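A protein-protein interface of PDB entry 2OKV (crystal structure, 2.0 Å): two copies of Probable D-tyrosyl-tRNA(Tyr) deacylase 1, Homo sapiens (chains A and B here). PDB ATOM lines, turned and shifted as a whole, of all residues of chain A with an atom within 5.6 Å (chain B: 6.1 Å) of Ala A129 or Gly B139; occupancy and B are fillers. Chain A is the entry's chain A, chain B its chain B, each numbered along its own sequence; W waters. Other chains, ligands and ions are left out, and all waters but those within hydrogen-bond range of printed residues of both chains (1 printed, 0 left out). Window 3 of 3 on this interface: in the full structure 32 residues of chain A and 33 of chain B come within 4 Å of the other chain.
The side-chain hydroxyl of Tyr A130 lies within hydrogen-bond range of the side-chain carboxylate of Asp B138 (2.5 Å). O of Met A131 is in hydrogen-bond range of N of Gly B139 (2.8 Å). NE2 of Gln A132 sits at hydrogen-bond distance from OD1 of Asp B138 (2.8 Å). O of Val A133 sits at hydrogen-bond distance from N of Asn B137.
The backbone NH (N) of Lys A126 sits at hydrogen-bond distance from the side-chain sulfur (SD) of Met A131 (3.5 Å). The backbone carbonyl oxygen (O) of Arg B7 sits close to the side-chain amide oxygen (OD1) of Asn B137 (3.3 Å). The guanidinium group of Arg B7 is in salt-bridge range of the side-chain carboxylate of Asp B138. The side-chain amide oxygen of Asn B137 is in hydrogen-bond range of the backbone NH of Val B141.
Ala A129 touches Gly B139. CE1 of Tyr A130 touches CA of Gly B139 (3.9 Å). O of Asn B137 touches O of Met A131, 3.7 Å away. Met A131 touches Asp B138. N of Pro B140 touches O of Met A131, 3.6 Å away. Asn B137 touches Gln A132 (O to CA, 3.5 Å). Val A133 touches Pro B140.
Ala A129 touches just one residue of chain B: Gly B139. Of chain A, only Ala A129 (3.9 Å), Tyr A130 (3.9 Å) and Met A131 (2.8 Å) come within 4 Å of Gly B139. Printed residues of chain B within 4 Å of Met A131: Asn B137, Asp B138, Gly B139 and Pro B140. Printed residues of chain A within 4 Å of Asn B137: Met A131 (3.7 Å), Gln A132 (3.5 Å) and Val A133 (2.8 Å). Of the printed residues of chain B, Val A133 touches Asn B137 and Pro B140. Of the printed residues of chain B, Tyr A130 touches Asp B138 (2.5 Å) and Gly B139 (3.9 Å). The nearest residue of chain B that does not touch Ala A129 is Pro B140 (5.5 Å). The nearest residue of chain A that does not touch Gly B139 is Gln A132 (4.3 Å). The nearest printed residue of chain B that does not touch Met A131 is Val B141 (6.4 Å).
Hydrophobic or aromatic side chains of chain A that line the printed part of chain B: Tyr A130, Met A131 and Val A133. Of the 6 printed residues of chain B, 4 touch a printed residue of chain A. Hydrophobic or aromatic side chains of chain B that line the printed part of chain A: Pro B140. Along chain B the printed residues that touch a printed residue of chain A span positions 137 to 140. Among the printed residues, 11 pairs touch across the chains.
No position is printed for both chains.
Water W1 lies within hydrogen-bond range of the backbone carbonyl oxygen of Ala A129 (2.6 Å) and the backbone carbonyl oxygen of Gly B139 (3.4 Å).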
ATOM      1  N   VAL A  15      23.774  17.484   7.442  1.00  0.00           N
ATOM      2  CA  VAL A  15      22.569  17.409   6.600  1.00  0.00           C
ATOM      3  C   VAL A  15      21.548  16.553   7.346  1.00  0.00           C
ATOM      4  O   VAL A  15      21.875  15.456   7.779  1.00  0.00           O
ATOM      5  CB  VAL A  15      22.870  16.780   5.210  1.00  0.00           C
ATOM      6  CG1 VAL A  15      21.599  16.608   4.401  1.00  0.00           C
ATOM      7  CG2 VAL A  15      23.909  17.619   4.451  1.00  0.00           C
ATOM      8  N   LYS A 126      27.787  18.237   0.713  1.00  0.00           N
ATOM      9  CA  LYS A 126      26.991  17.358  -0.137  1.00  0.00           C
ATOM     10  C   LYS A 126      26.260  18.235  -1.143  1.00  0.00           C
ATOM     11  O   LYS A 126      25.238  18.838  -0.836  1.00  0.00           O
ATOM     12  CB  LYS A 126      26.008  16.536   0.695  1.00  0.00           C
ATOM     13  CG  LYS A 126      25.425  15.300  -0.022  1.00  0.00           C
ATOM     14  CD  LYS A 126      24.562  14.540   0.953  1.00  0.00           C
ATOM     15  CE  LYS A 126      24.407  13.085   0.572  1.00  0.00           C
ATOM     16  NZ  LYS A 126      23.097  12.853  -0.008  1.00  0.00           N
ATOM     17  N   PHE A 127      26.800  18.278  -2.354  1.00  0.00           N
ATOM     18  CA  PHE A 127      26.385  19.225  -3.378  1.00  0.00           C
ATOM     19  C   PHE A 127      24.868  19.484  -3.427  1.00  0.00           C
ATOM     20  O   PHE A 127      24.428  20.626  -3.318  1.00  0.00           O
ATOM     21  CB  PHE A 127      26.962  18.823  -4.743  1.00  0.00           C
ATOM     22  CG  PHE A 127      26.681  19.817  -5.823  1.00  0.00           C
ATOM     23  CD1 PHE A 127      27.598  20.824  -6.121  1.00  0.00           C
ATOM     24  CD2 PHE A 127      25.479  19.778  -6.507  1.00  0.00           C
ATOM     25  CE1 PHE A 127      27.314  21.758  -7.117  1.00  0.00           C
ATOM     26  CE2 PHE A 127      25.191  20.707  -7.493  1.00  0.00           C
ATOM     27  CZ  PHE A 127      26.116  21.703  -7.789  1.00  0.00           C
ATOM     28  N   GLY A 128      24.044  18.461  -3.536  1.00  0.00           N
ATOM     29  CA  GLY A 128      22.591  18.771  -3.613  1.00  0.00           C
ATOM     30  C   GLY A 128      21.928  19.459  -2.407  1.00  0.00           C
ATOM     31  O   GLY A 128      20.909  20.162  -2.551  1.00  0.00           O
ATOM     32  N   ALA A 129      22.520  19.269  -1.231  1.00  0.00           N
ATOM     33  CA  ALA A 129      21.788  19.248   0.036  1.00  0.00           C
ATOM     34  C   ALA A 129      21.609  20.568   0.766  1.00  0.00           C
ATOM     35  O   ALA A 129      22.387  21.503   0.576  1.00  0.00           O
ATOM     36  CB  ALA A 129      22.438  18.219   0.972  1.00  0.00           C
ATOM     37  N   TYR A 130      20.581  20.621   1.616  1.00  0.00           N
ATOM     38  CA  TYR A 130      20.411  21.679   2.606  1.00  0.00           C
ATOM     39  C   TYR A 130      21.352  21.430   3.783  1.00  0.00           C
ATOM     40  O   TYR A 130      21.086  20.569   4.623  1.00  0.00           O
ATOM     41  CB  TYR A 130      18.953  21.741   3.094  1.00  0.00           C
ATOM     42  CG  TYR A 130      18.666  22.755   4.205  1.00  0.00           C
ATOM     43  CD1 TYR A 130      19.235  24.023   4.194  1.00  0.00           C
ATOM     44  CD2 TYR A 130      17.752  22.460   5.234  1.00  0.00           C
ATOM     45  CE1 TYR A 130      18.958  24.964   5.198  1.00  0.00           C
ATOM     46  CE2 TYR A 130      17.454  23.401   6.249  1.00  0.00           C
ATOM     47  CZ  TYR A 130      18.066  24.652   6.217  1.00  0.00           C
ATOM     48  OH  TYR A 130      17.785  25.592   7.204  1.00  0.00           O
ATOM     49  N   MET A 131      22.437  22.197   3.847  1.00  0.00           N
ATOM     50  CA  MET A 131      23.513  21.969   4.818  1.00  0.00           C
ATOM     51  C   MET A 131      23.570  23.051   5.896  1.00  0.00           C
ATOM     52  O   MET A 131      23.309  24.229   5.618  1.00  0.00           O
ATOM     53  CB  MET A 131      24.864  21.965   4.112  1.00  0.00           C
ATOM     54  CG  MET A 131      25.092  20.853   3.090  1.00  0.00           C
ATOM     55  SD  MET A 131      26.595  21.194   2.161  1.00  0.00           S
ATOM     56  CE  MET A 131      25.898  21.998   0.715  1.00  0.00           C
ATOM     57  N   GLN A 132      23.887  22.632   7.118  1.00  0.00           N
ATOM     58  CA  GLN A 132      24.462  23.525   8.130  1.00  0.00           C
ATOM     59  C   GLN A 132      25.977  23.415   8.058  1.00  0.00           C
ATOM     60  O   GLN A 132      26.538  22.332   8.264  1.00  0.00           O
ATOM     61  CB  GLN A 132      23.975  23.155   9.536  1.00  0.00           C
ATOM     62  CG  GLN A 132      22.465  23.056   9.635  1.00  0.00           C
ATOM     63  CD  GLN A 132      21.795  24.418   9.494  1.00  0.00           C
ATOM     64  OE1 GLN A 132      22.094  25.344  10.242  1.00  0.00           O
ATOM     65  NE2 GLN A 132      20.923  24.546   8.522  1.00  0.00           N
ATOM     66  N   VAL A 133      26.649  24.529   7.772  1.00  0.00           N
ATOM     67  CA  VAL A 133      28.102  24.515   7.688  1.00  0.00           C
ATOM     68  C   VAL A 133      28.611  25.217   8.943  1.00  0.00           C
ATOM     69  O   VAL A 133      28.470  26.438   9.095  1.00  0.00           O
ATOM     70  CB  VAL A 133      28.611  25.162   6.380  1.00  0.00           C
ATOM     71  CG1 VAL A 133      30.160  25.028   6.264  1.00  0.00           C
ATOM     72  CG2 VAL A 133      27.897  24.516   5.143  1.00  0.00           C
ATOM     73  N   ARG B   7      24.217  33.819   6.443  1.00  0.00           N
ATOM     74  CA  ARG B   7      22.956  33.554   7.126  1.00  0.00           C
ATOM     75  C   ARG B   7      23.220  32.460   8.143  1.00  0.00           C
ATOM     76  O   ARG B   7      23.790  31.433   7.803  1.00  0.00           O
ATOM     77  CB  ARG B   7      21.875  33.101   6.139  1.00  0.00           C
ATOM     78  CG  ARG B   7      20.532  32.773   6.802  1.00  0.00           C
ATOM     79  CD  ARG B   7      19.453  32.403   5.801  1.00  0.00           C
ATOM     80  NE  ARG B   7      19.648  31.055   5.265  1.00  0.00           N
ATOM     81  CZ  ARG B   7      18.849  30.471   4.382  1.00  0.00           C
ATOM     82  NH1 ARG B   7      17.796  31.124   3.893  1.00  0.00           N
ATOM     83  NH2 ARG B   7      19.115  29.231   3.970  1.00  0.00           N
ATOM     84  N   ASN B 137      26.497  28.409   9.517  1.00  0.00           N
ATOM     85  CA  ASN B 137      25.995  28.958   8.269  1.00  0.00           C
ATOM     86  C   ASN B 137      24.831  28.094   7.766  1.00  0.00           C
ATOM     87  O   ASN B 137      25.012  26.917   7.472  1.00  0.00           O
ATOM     88  CB  ASN B 137      27.131  29.044   7.243  1.00  0.00           C
ATOM     89  CG  ASN B 137      26.752  29.859   5.997  1.00  0.00           C
ATOM     90  OD1 ASN B 137      25.622  29.825   5.540  1.00  0.00           O
ATOM     91  ND2 ASN B 137      27.710  30.606   5.461  1.00  0.00           N
ATOM     92  N   ASP B 138      23.651  28.706   7.690  1.00  0.00           N
ATOM     93  CA  ASP B 138      22.376  28.022   7.401  1.00  0.00           C
ATOM     94  C   ASP B 138      22.095  27.993   5.906  1.00  0.00           C
ATOM     95  O   ASP B 138      21.591  28.976   5.347  1.00  0.00           O
ATOM     96  CB  ASP B 138      21.272  28.766   8.141  1.00  0.00           C
ATOM     97  CG  ASP B 138      19.912  28.180   7.933  1.00  0.00           C
ATOM     98  OD1 ASP B 138      19.790  26.964   7.683  1.00  0.00           O
ATOM     99  OD2 ASP B 138      18.949  28.962   8.058  1.00  0.00           O
ATOM    100  N   GLY B 139      22.451  26.873   5.260  1.00  0.00           N
ATOM    101  CA  GLY B 139      22.190  26.683   3.832  1.00  0.00           C
ATOM    102  C   GLY B 139      23.238  25.882   3.070  1.00  0.00           C
ATOM    103  O   GLY B 139      22.950  24.790   2.567  1.00  0.00           O
ATOM    104  N   PRO B 140      24.467  26.420   2.951  1.00  0.00           N
ATOM    105  CA  PRO B 140      24.922  27.707   3.442  1.00  0.00           C
ATOM    106  C   PRO B 140      24.375  28.831   2.545  1.00  0.00           C
ATOM    107  O   PRO B 140      24.009  28.572   1.401  1.00  0.00           O
ATOM    108  CB  PRO B 140      26.451  27.606   3.326  1.00  0.00           C
ATOM    109  CG  PRO B 140      26.680  26.685   2.162  1.00  0.00           C
ATOM    110  CD  PRO B 140      25.519  25.693   2.204  1.00  0.00           C
ATOM    111  N   VAL B 141      24.303  30.046   3.084  1.00  0.00           N
ATOM    112  CA  VAL B 141      23.974  31.249   2.292  1.00  0.00           C
ATOM    113  C   VAL B 141      25.025  32.299   2.642  1.00  0.00           C
ATOM    114  O   VAL B 141      25.207  32.649   3.825  1.00  0.00           O
ATOM    115  CB  VAL B 141      22.551  31.793   2.578  1.00  0.00           C
ATOM    116  CG1 VAL B 141      22.357  33.161   1.925  1.00  0.00           C
ATOM    117  CG2 VAL B 141      21.508  30.843   2.042  1.00  0.00           C
HETATM  118  O   HOH W   1      23.207  23.600  -0.655  1.00  0.00           O
